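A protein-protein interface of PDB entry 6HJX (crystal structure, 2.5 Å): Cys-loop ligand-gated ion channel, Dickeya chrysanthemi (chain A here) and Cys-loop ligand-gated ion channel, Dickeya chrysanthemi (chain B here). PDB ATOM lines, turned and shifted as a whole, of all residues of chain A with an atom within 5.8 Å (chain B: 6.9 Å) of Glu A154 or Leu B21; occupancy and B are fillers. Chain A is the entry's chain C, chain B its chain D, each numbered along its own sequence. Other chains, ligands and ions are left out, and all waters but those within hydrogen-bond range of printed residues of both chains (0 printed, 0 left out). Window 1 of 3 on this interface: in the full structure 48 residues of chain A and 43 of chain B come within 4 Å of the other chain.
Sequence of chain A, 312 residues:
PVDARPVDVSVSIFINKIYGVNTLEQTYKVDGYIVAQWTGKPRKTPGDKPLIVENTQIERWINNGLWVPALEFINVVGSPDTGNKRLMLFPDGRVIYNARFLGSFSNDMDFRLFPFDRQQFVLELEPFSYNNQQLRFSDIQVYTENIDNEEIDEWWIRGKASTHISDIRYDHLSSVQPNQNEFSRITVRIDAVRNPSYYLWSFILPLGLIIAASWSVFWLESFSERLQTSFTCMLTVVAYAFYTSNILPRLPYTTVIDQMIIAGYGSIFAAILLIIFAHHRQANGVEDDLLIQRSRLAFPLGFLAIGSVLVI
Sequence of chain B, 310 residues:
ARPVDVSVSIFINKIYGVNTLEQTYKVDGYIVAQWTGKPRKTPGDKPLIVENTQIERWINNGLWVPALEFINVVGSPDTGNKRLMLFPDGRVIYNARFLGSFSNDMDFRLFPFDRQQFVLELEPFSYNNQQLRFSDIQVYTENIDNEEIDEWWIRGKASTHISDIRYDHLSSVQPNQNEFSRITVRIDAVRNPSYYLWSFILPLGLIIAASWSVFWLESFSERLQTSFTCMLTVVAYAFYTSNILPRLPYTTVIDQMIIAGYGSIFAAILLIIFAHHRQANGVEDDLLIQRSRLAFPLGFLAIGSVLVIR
NH1 of Arg A194 lies within salt-bridge range of OE2 of Glu A154 (3.7 Å).
The backbone NH of Phe B108 is in hydrogen-bond range of the side-chain hydroxyl of Tyr B250 (2.8 Å).
The side-chain amide oxygen (OD1) of Asn B19 sits at hydrogen-bond distance from the backbone NH (N) of Leu B21 (3.1 Å).
The backbone NH of Asn A195 lies within hydrogen-bond range of the backbone carbonyl oxygen of Glu A154, at 2.8 Å.
Among the printed residues, pairs that only touch across the chains: Glu A154 with Leu B21, Asn A195 with Pro B249, Ile A152 with Tyr B250 and Glu A154 with Pro B249.
Of chain A, only Glu A154 comes within 4 Å of Leu B21.
Of the printed residues of chain B, Ile A152 touches Tyr B250 (3.6 Å).
Printed residues of chain B within 4 Å of Asn A195: Pro B249 (3.5 Å).
Arg B247 touches none of the printed residues of chain A.
Arg A194 touches none of the printed residues of chain B.
Of the 13 printed residues of chain B, 3 touch a printed residue of chain A.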
ATOM      1  N   VAL A  21       1.694  12.380 -21.625  1.00  0.00           N
ATOM      2  CA  VAL A  21       2.347  12.113 -22.899  1.00  0.00           C
ATOM      3  C   VAL A  21       3.835  12.393 -22.765  1.00  0.00           C
ATOM      4  O   VAL A  21       4.242  13.449 -22.267  1.00  0.00           O
ATOM      5  CB  VAL A  21       1.722  12.960 -24.018  1.00  0.00           C
ATOM      6  CG1 VAL A  21       2.513  12.806 -25.316  1.00  0.00           C
ATOM      7  CG2 VAL A  21       0.270  12.568 -24.238  1.00  0.00           C
ATOM      8  N   GLU A 150     -14.061  21.650 -22.371  1.00  0.00           N
ATOM      9  CA  GLU A 150     -12.805  21.177 -22.940  1.00  0.00           C
ATOM     10  C   GLU A 150     -11.757  22.273 -23.097  1.00  0.00           C
ATOM     11  O   GLU A 150     -10.604  21.960 -23.415  1.00  0.00           O
ATOM     12  CB  GLU A 150     -13.060  20.522 -24.304  1.00  0.00           C
ATOM     13  CG  GLU A 150     -13.642  21.454 -25.357  1.00  0.00           C
ATOM     14  CD  GLU A 150     -13.990  20.731 -26.643  1.00  0.00           C
ATOM     15  OE1 GLU A 150     -13.894  19.486 -26.670  1.00  0.00           O
ATOM     16  OE2 GLU A 150     -14.362  21.405 -27.627  1.00  0.00           O
ATOM     17  N   ILE A 152     -10.192  23.832 -20.925  1.00  0.00           N
ATOM     18  CA  ILE A 152      -9.137  23.694 -19.924  1.00  0.00           C
ATOM     19  C   ILE A 152      -8.254  22.477 -20.161  1.00  0.00           C
ATOM     20  O   ILE A 152      -7.173  22.379 -19.559  1.00  0.00           O
ATOM     21  CB  ILE A 152      -9.750  23.621 -18.508  1.00  0.00           C
ATOM     22  CG1 ILE A 152      -8.655  23.669 -17.441  1.00  0.00           C
ATOM     23  CG2 ILE A 152     -10.590  22.355 -18.353  1.00  0.00           C
ATOM     24  CD1 ILE A 152      -9.181  23.864 -16.033  1.00  0.00           C
ATOM     25  N   ASP A 153      -8.668  21.554 -21.024  1.00  0.00           N
ATOM     26  CA  ASP A 153      -7.954  20.300 -21.214  1.00  0.00           C
ATOM     27  C   ASP A 153      -6.929  20.414 -22.335  1.00  0.00           C
ATOM     28  O   ASP A 153      -7.137  21.109 -23.334  1.00  0.00           O
ATOM     29  CB  ASP A 153      -8.937  19.171 -21.523  1.00  0.00           C
ATOM     30  CG  ASP A 153      -9.950  18.963 -20.417  1.00  0.00           C
ATOM     31  OD1 ASP A 153      -9.571  19.081 -19.232  1.00  0.00           O
ATOM     32  OD2 ASP A 153     -11.125  18.690 -20.732  1.00  0.00           O
ATOM     33  N   GLU A 154      -5.812  19.705 -22.156  1.00  0.00           N
ATOM     34  CA  GLU A 154      -4.732  19.741 -23.134  1.00  0.00           C
ATOM     35  C   GLU A 154      -5.158  19.127 -24.462  1.00  0.00           C
ATOM     36  O   GLU A 154      -4.731  19.592 -25.527  1.00  0.00           O
ATOM     37  CB  GLU A 154      -3.510  19.016 -22.568  1.00  0.00           C
ATOM     38  CG  GLU A 154      -2.252  19.123 -23.413  1.00  0.00           C
ATOM     39  CD  GLU A 154      -1.032  18.547 -22.709  1.00  0.00           C
ATOM     40  OE1 GLU A 154      -1.021  18.521 -21.461  1.00  0.00           O
ATOM     41  OE2 GLU A 154      -0.087  18.116 -23.402  1.00  0.00           O
ATOM     42  N   TRP A 155      -6.001  18.097 -24.423  1.00  0.00           N
ATOM     43  CA  TRP A 155      -6.424  17.381 -25.618  1.00  0.00           C
ATOM     44  C   TRP A 155      -7.944  17.372 -25.710  1.00  0.00           C
ATOM     45  O   TRP A 155      -8.643  17.387 -24.693  1.00  0.00           O
ATOM     46  CB  TRP A 155      -5.894  15.937 -25.617  1.00  0.00           C
ATOM     47  CG  TRP A 155      -4.394  15.833 -25.588  1.00  0.00           C
ATOM     48  CD1 TRP A 155      -3.595  15.828 -24.481  1.00  0.00           C
ATOM     49  CD2 TRP A 155      -3.518  15.711 -26.715  1.00  0.00           C
ATOM     50  NE1 TRP A 155      -2.276  15.714 -24.850  1.00  0.00           N
ATOM     51  CE2 TRP A 155      -2.203  15.639 -26.215  1.00  0.00           C
ATOM     52  CE3 TRP A 155      -3.720  15.655 -28.099  1.00  0.00           C
ATOM     53  CZ2 TRP A 155      -1.093  15.517 -27.050  1.00  0.00           C
ATOM     54  CZ3 TRP A 155      -2.616  15.534 -28.925  1.00  0.00           C
ATOM     55  CH2 TRP A 155      -1.321  15.467 -28.399  1.00  0.00           C
ATOM     56  N   TRP A 156      -8.448  17.348 -26.943  1.00  0.00           N
ATOM     57  CA  TRP A 156      -9.880  17.336 -27.220  1.00  0.00           C
ATOM     58  C   TRP A 156     -10.221  16.046 -27.952  1.00  0.00           C
ATOM     59  O   TRP A 156      -9.656  15.764 -29.015  1.00  0.00           O
ATOM     60  CB  TRP A 156     -10.294  18.551 -28.054  1.00  0.00           C
ATOM     61  CG  TRP A 156      -9.959  19.871 -27.426  1.00  0.00           C
ATOM     62  CD1 TRP A 156      -9.775  20.127 -26.098  1.00  0.00           C
ATOM     63  CD2 TRP A 156      -9.761  21.116 -28.106  1.00  0.00           C
ATOM     64  NE1 TRP A 156      -9.477  21.456 -25.909  1.00  0.00           N
ATOM     65  CE2 TRP A 156      -9.462  22.084 -27.127  1.00  0.00           C
ATOM     66  CE3 TRP A 156      -9.807  21.507 -29.449  1.00  0.00           C
ATOM     67  CZ2 TRP A 156      -9.211  23.418 -27.447  1.00  0.00           C
ATOM     68  CZ3 TRP A 156      -9.558  22.830 -29.763  1.00  0.00           C
ATOM     69  CH2 TRP A 156      -9.263  23.768 -28.767  1.00  0.00           C
ATOM     70  N   VAL A 193      -7.157  15.665 -30.419  1.00  0.00           N
ATOM     71  CA  VAL A 193      -6.525  16.805 -31.071  1.00  0.00           C
ATOM     72  C   VAL A 193      -5.990  17.731 -29.989  1.00  0.00           C
ATOM     73  O   VAL A 193      -6.669  17.990 -28.991  1.00  0.00           O
ATOM     74  CB  VAL A 193      -7.512  17.553 -31.992  1.00  0.00           C
ATOM     75  CG1 VAL A 193      -6.807  18.681 -32.735  1.00  0.00           C
ATOM     76  CG2 VAL A 193      -8.158  16.584 -32.970  1.00  0.00           C
ATOM     77  N   ARG A 194      -4.773  18.227 -30.185  1.00  0.00           N
ATOM     78  CA  ARG A 194      -4.152  19.086 -29.189  1.00  0.00           C
ATOM     79  C   ARG A 194      -4.854  20.440 -29.128  1.00  0.00           C
ATOM     80  O   ARG A 194      -5.458  20.898 -30.101  1.00  0.00           O
ATOM     81  CB  ARG A 194      -2.667  19.285 -29.505  1.00  0.00           C
ATOM     82  CG  ARG A 194      -1.898  20.040 -28.429  1.00  0.00           C
ATOM     83  CD  ARG A 194      -0.460  20.303 -28.848  1.00  0.00           C
ATOM     84  NE  ARG A 194       0.250  19.069 -29.176  1.00  0.00           N
ATOM     85  CZ  ARG A 194       0.824  18.270 -28.282  1.00  0.00           C
ATOM     86  NH1 ARG A 194       0.778  18.562 -26.990  1.00  0.00           N
ATOM     87  NH2 ARG A 194       1.445  17.170 -28.683  1.00  0.00           N
ATOM     88  N   ASN A 195      -4.772  21.075 -27.958  1.00  0.00           N
ATOM     89  CA  ASN A 195      -5.290  22.421 -27.753  1.00  0.00           C
ATOM     90  C   ASN A 195      -4.223  23.442 -28.139  1.00  0.00           C
ATOM     91  O   ASN A 195      -3.328  23.731 -27.335  1.00  0.00           O
ATOM     92  CB  ASN A 195      -5.708  22.617 -26.293  1.00  0.00           C
ATOM     93  CG  ASN A 195      -6.103  24.050 -25.987  1.00  0.00           C
ATOM     94  OD1 ASN A 195      -6.643  24.754 -26.841  1.00  0.00           O
ATOM     95  ND2 ASN A 195      -5.826  24.491 -24.764  1.00  0.00           N
ATOM     96  N   TYR A 199      -0.083  27.569 -27.183  1.00  0.00           N
ATOM     97  CA  TYR A 199       1.091  27.701 -28.037  1.00  0.00           C
ATOM     98  C   TYR A 199       0.954  28.828 -29.050  1.00  0.00           C
ATOM     99  O   TYR A 199       1.972  29.357 -29.510  1.00  0.00           O
ATOM    100  CB  TYR A 199       1.364  26.373 -28.751  1.00  0.00           C
ATOM    101  CG  TYR A 199       1.437  25.195 -27.802  1.00  0.00           C
ATOM    102  CD1 TYR A 199       2.531  25.018 -26.967  1.00  0.00           C
ATOM    103  CD2 TYR A 199       0.403  24.269 -27.731  1.00  0.00           C
ATOM    104  CE1 TYR A 199       2.598  23.951 -26.091  1.00  0.00           C
ATOM    105  CE2 TYR A 199       0.462  23.199 -26.859  1.00  0.00           C
ATOM    106  CZ  TYR A 199       1.562  23.046 -26.042  1.00  0.00           C
ATOM    107  OH  TYR A 199       1.629  21.983 -25.171  1.00  0.00           O
ATOM    108  N   VAL B  18       1.907  19.125  -5.750  1.00  0.00           N
ATOM    109  CA  VAL B  18       0.987  19.371  -6.851  1.00  0.00           C
ATOM    110  C   VAL B  18       1.727  19.241  -8.173  1.00  0.00           C
ATOM    111  O   VAL B  18       2.798  19.830  -8.364  1.00  0.00           O
ATOM    112  CB  VAL B  18       0.349  20.761  -6.711  1.00  0.00           C
ATOM    113  CG1 VAL B  18      -0.497  21.088  -7.931  1.00  0.00           C
ATOM    114  CG2 VAL B  18      -0.482  20.838  -5.443  1.00  0.00           C
ATOM    115  N   ASN B  19       1.156  18.473  -9.093  1.00  0.00           N
ATOM    116  CA  ASN B  19       1.648  18.380 -10.467  1.00  0.00           C
ATOM    117  C   ASN B  19       0.633  19.106 -11.343  1.00  0.00           C
ATOM    118  O   ASN B  19      -0.401  18.541 -11.706  1.00  0.00           O
ATOM    119  CB  ASN B  19       1.827  16.928 -10.897  1.00  0.00           C
ATOM    120  CG  ASN B  19       2.446  16.800 -12.279  1.00  0.00           C
ATOM    121  OD1 ASN B  19       2.147  17.582 -13.185  1.00  0.00           O
ATOM    122  ND2 ASN B  19       3.318  15.812 -12.444  1.00  0.00           N
ATOM    123  N   THR B  20       0.931  20.365 -11.673  1.00  0.00           N
ATOM    124  CA  THR B  20      -0.022  21.187 -12.413  1.00  0.00           C
ATOM    125  C   THR B  20      -0.404  20.543 -13.738  1.00  0.00           C
ATOM    126  O   THR B  20      -1.581  20.535 -14.119  1.00  0.00           O
ATOM    127  CB  THR B  20       0.565  22.578 -12.650  1.00  0.00           C
ATOM    128  OG1 THR B  20       1.904  22.452 -13.143  1.00  0.00           O
ATOM    129  CG2 THR B  20       0.574  23.385 -11.363  1.00  0.00           C
ATOM    130  N   LEU B  21       0.576  19.992 -14.457  1.00  0.00           N
ATOM    131  CA  LEU B  21       0.298  19.443 -15.779  1.00  0.00           C
ATOM    132  C   LEU B  21      -0.616  18.226 -15.692  1.00  0.00           C
ATOM    133  O   LEU B  21      -1.545  18.082 -16.496  1.00  0.00           O
ATOM    134  CB  LEU B  21       1.607  19.086 -16.480  1.00  0.00           C
ATOM    135  CG  LEU B  21       1.474  18.606 -17.925  1.00  0.00           C
ATOM    136  CD1 LEU B  21       0.878  19.694 -18.802  1.00  0.00           C
ATOM    137  CD2 LEU B  21       2.826  18.161 -18.458  1.00  0.00           C
ATOM    138  N   GLU B  22      -0.373  17.344 -14.726  1.00  0.00           N
ATOM    139  CA  GLU B  22      -1.172  16.137 -14.565  1.00  0.00           C
ATOM    140  C   GLU B  22      -2.387  16.338 -13.672  1.00  0.00           C
ATOM    141  O   GLU B  22      -3.236  15.445 -13.596  1.00  0.00           O
ATOM    142  CB  GLU B  22      -0.303  15.008 -14.001  1.00  0.00           C
ATOM    143  CG  GLU B  22       0.875  14.645 -14.898  1.00  0.00           C
ATOM    144  CD  GLU B  22       1.654  13.444 -14.397  1.00  0.00           C
ATOM    145  OE1 GLU B  22       1.501  13.077 -13.210  1.00  0.00           O
ATOM    146  OE2 GLU B  22       2.419  12.863 -15.197  1.00  0.00           O
ATOM    147  N   GLN B  23      -2.500  17.490 -13.013  1.00  0.00           N
ATOM    148  CA  GLN B  23      -3.588  17.767 -12.078  1.00  0.00           C
ATOM    149  C   GLN B  23      -3.667  16.691 -10.992  1.00  0.00           C
ATOM    150  O   GLN B  23      -4.698  16.054 -10.778  1.00  0.00           O
ATOM    151  CB  GLN B  23      -4.918  17.897 -12.823  1.00  0.00           C
ATOM    152  CG  GLN B  23      -4.960  19.081 -13.779  1.00  0.00           C
ATOM    153  CD  GLN B  23      -6.213  19.104 -14.624  1.00  0.00           C
ATOM    154  OE1 GLN B  23      -7.323  19.212 -14.107  1.00  0.00           O
ATOM    155  NE2 GLN B  23      -6.042  18.996 -15.937  1.00  0.00           N
ATOM    156  N   THR B  24      -2.551  16.514 -10.292  1.00  0.00           N
ATOM    157  CA  THR B  24      -2.454  15.523  -9.232  1.00  0.00           C
ATOM    158  C   THR B  24      -1.800  16.148  -8.010  1.00  0.00           C
ATOM    159  O   THR B  24      -1.172  17.209  -8.083  1.00  0.00           O
ATOM    160  CB  THR B  24      -1.652  14.287  -9.671  1.00  0.00           C
ATOM    161  OG1 THR B  24      -0.290  14.658  -9.920  1.00  0.00           O
ATOM    162  CG2 THR B  24      -2.256  13.668 -10.930  1.00  0.00           C
ATOM    163  N   PHE B 108      -5.687  26.581 -13.015  1.00  0.00           N
ATOM    164  CA  PHE B 108      -4.622  27.488 -12.605  1.00  0.00           C
ATOM    165  C   PHE B 108      -4.614  28.774 -13.429  1.00  0.00           C
ATOM    166  O   PHE B 108      -3.576  29.430 -13.553  1.00  0.00           O
ATOM    167  CB  PHE B 108      -3.264  26.791 -12.708  1.00  0.00           C
ATOM    168  CG  PHE B 108      -3.172  25.509 -11.923  1.00  0.00           C
ATOM    169  CD1 PHE B 108      -2.834  25.525 -10.581  1.00  0.00           C
ATOM    170  CD2 PHE B 108      -3.418  24.288 -12.531  1.00  0.00           C
ATOM    171  CE1 PHE B 108      -2.748  24.348  -9.857  1.00  0.00           C
ATOM    172  CE2 PHE B 108      -3.331  23.109 -11.815  1.00  0.00           C
ATOM    173  CZ  PHE B 108      -2.996  23.138 -10.476  1.00  0.00           C
ATOM    174  N   PRO B 246       4.676  27.172 -13.085  1.00  0.00           N
ATOM    175  CA  PRO B 246       4.350  25.787 -13.438  1.00  0.00           C
ATOM    176  C   PRO B 246       4.049  25.626 -14.920  1.00  0.00           C
ATOM    177  O   PRO B 246       3.651  26.562 -15.616  1.00  0.00           O
ATOM    178  CB  PRO B 246       3.111  25.486 -12.587  1.00  0.00           C
ATOM    179  CG  PRO B 246       2.479  26.818 -12.364  1.00  0.00           C
ATOM    180  CD  PRO B 246       3.617  27.798 -12.270  1.00  0.00           C
ATOM    181  N   ARG B 247       4.258  24.402 -15.399  1.00  0.00           N
ATOM    182  CA  ARG B 247       3.934  24.048 -16.775  1.00  0.00           C
ATOM    183  C   ARG B 247       2.433  23.810 -16.888  1.00  0.00           C
ATOM    184  O   ARG B 247       1.872  22.993 -16.151  1.00  0.00           O
ATOM    185  CB  ARG B 247       4.720  22.809 -17.201  1.00  0.00           C
ATOM    186  N   LEU B 248       1.784  24.528 -17.798  1.00  0.00           N
ATOM    187  CA  LEU B 248       0.338  24.467 -17.964  1.00  0.00           C
ATOM    188  C   LEU B 248      -0.009  24.409 -19.442  1.00  0.00           C
ATOM    189  O   LEU B 248       0.751  24.905 -20.282  1.00  0.00           O
ATOM    190  CB  LEU B 248      -0.353  25.684 -17.331  1.00  0.00           C
ATOM    191  CG  LEU B 248      -0.284  25.776 -15.807  1.00  0.00           C
ATOM    192  CD1 LEU B 248      -0.748  27.144 -15.335  1.00  0.00           C
ATOM    193  CD2 LEU B 248      -1.123  24.676 -15.171  1.00  0.00           C
ATOM    194  N   PRO B 249      -1.154  23.812 -19.791  1.00  0.00           N
ATOM    195  CA  PRO B 249      -1.575  23.793 -21.199  1.00  0.00           C
ATOM    196  C   PRO B 249      -2.398  25.012 -21.591  1.00  0.00           C
ATOM    197  O   PRO B 249      -3.065  25.010 -22.630  1.00  0.00           O
ATOM    198  CB  PRO B 249      -2.400  22.503 -21.288  1.00  0.00           C
ATOM    199  CG  PRO B 249      -3.011  22.377 -19.928  1.00  0.00           C
ATOM    200  CD  PRO B 249      -2.022  22.966 -18.947  1.00  0.00           C
ATOM    201  N   TYR B 250      -2.364  26.055 -20.764  1.00  0.00           N
ATOM    202  CA  TYR B 250      -3.082  27.288 -21.052  1.00  0.00           C
ATOM    203  C   TYR B 250      -2.344  28.455 -20.409  1.00  0.00           C
ATOM    204  O   TYR B 250      -1.413  28.272 -19.620  1.00  0.00           O
ATOM    205  CB  TYR B 250      -4.535  27.220 -20.566  1.00  0.00           C
ATOM    206  CG  TYR B 250      -4.699  26.648 -19.179  1.00  0.00           C
ATOM    207  CD1 TYR B 250      -4.507  27.438 -18.053  1.00  0.00           C
ATOM    208  CD2 TYR B 250      -5.056  25.320 -18.996  1.00  0.00           C
ATOM    209  CE1 TYR B 250      -4.658  26.915 -16.782  1.00  0.00           C
ATOM    210  CE2 TYR B 250      -5.211  24.791 -17.731  1.00  0.00           C
ATOM    211  CZ  TYR B 250      -5.012  25.594 -16.628  1.00  0.00           C
ATOM    212  OH  TYR B 250      -5.165  25.072 -15.366  1.00  0.00           O
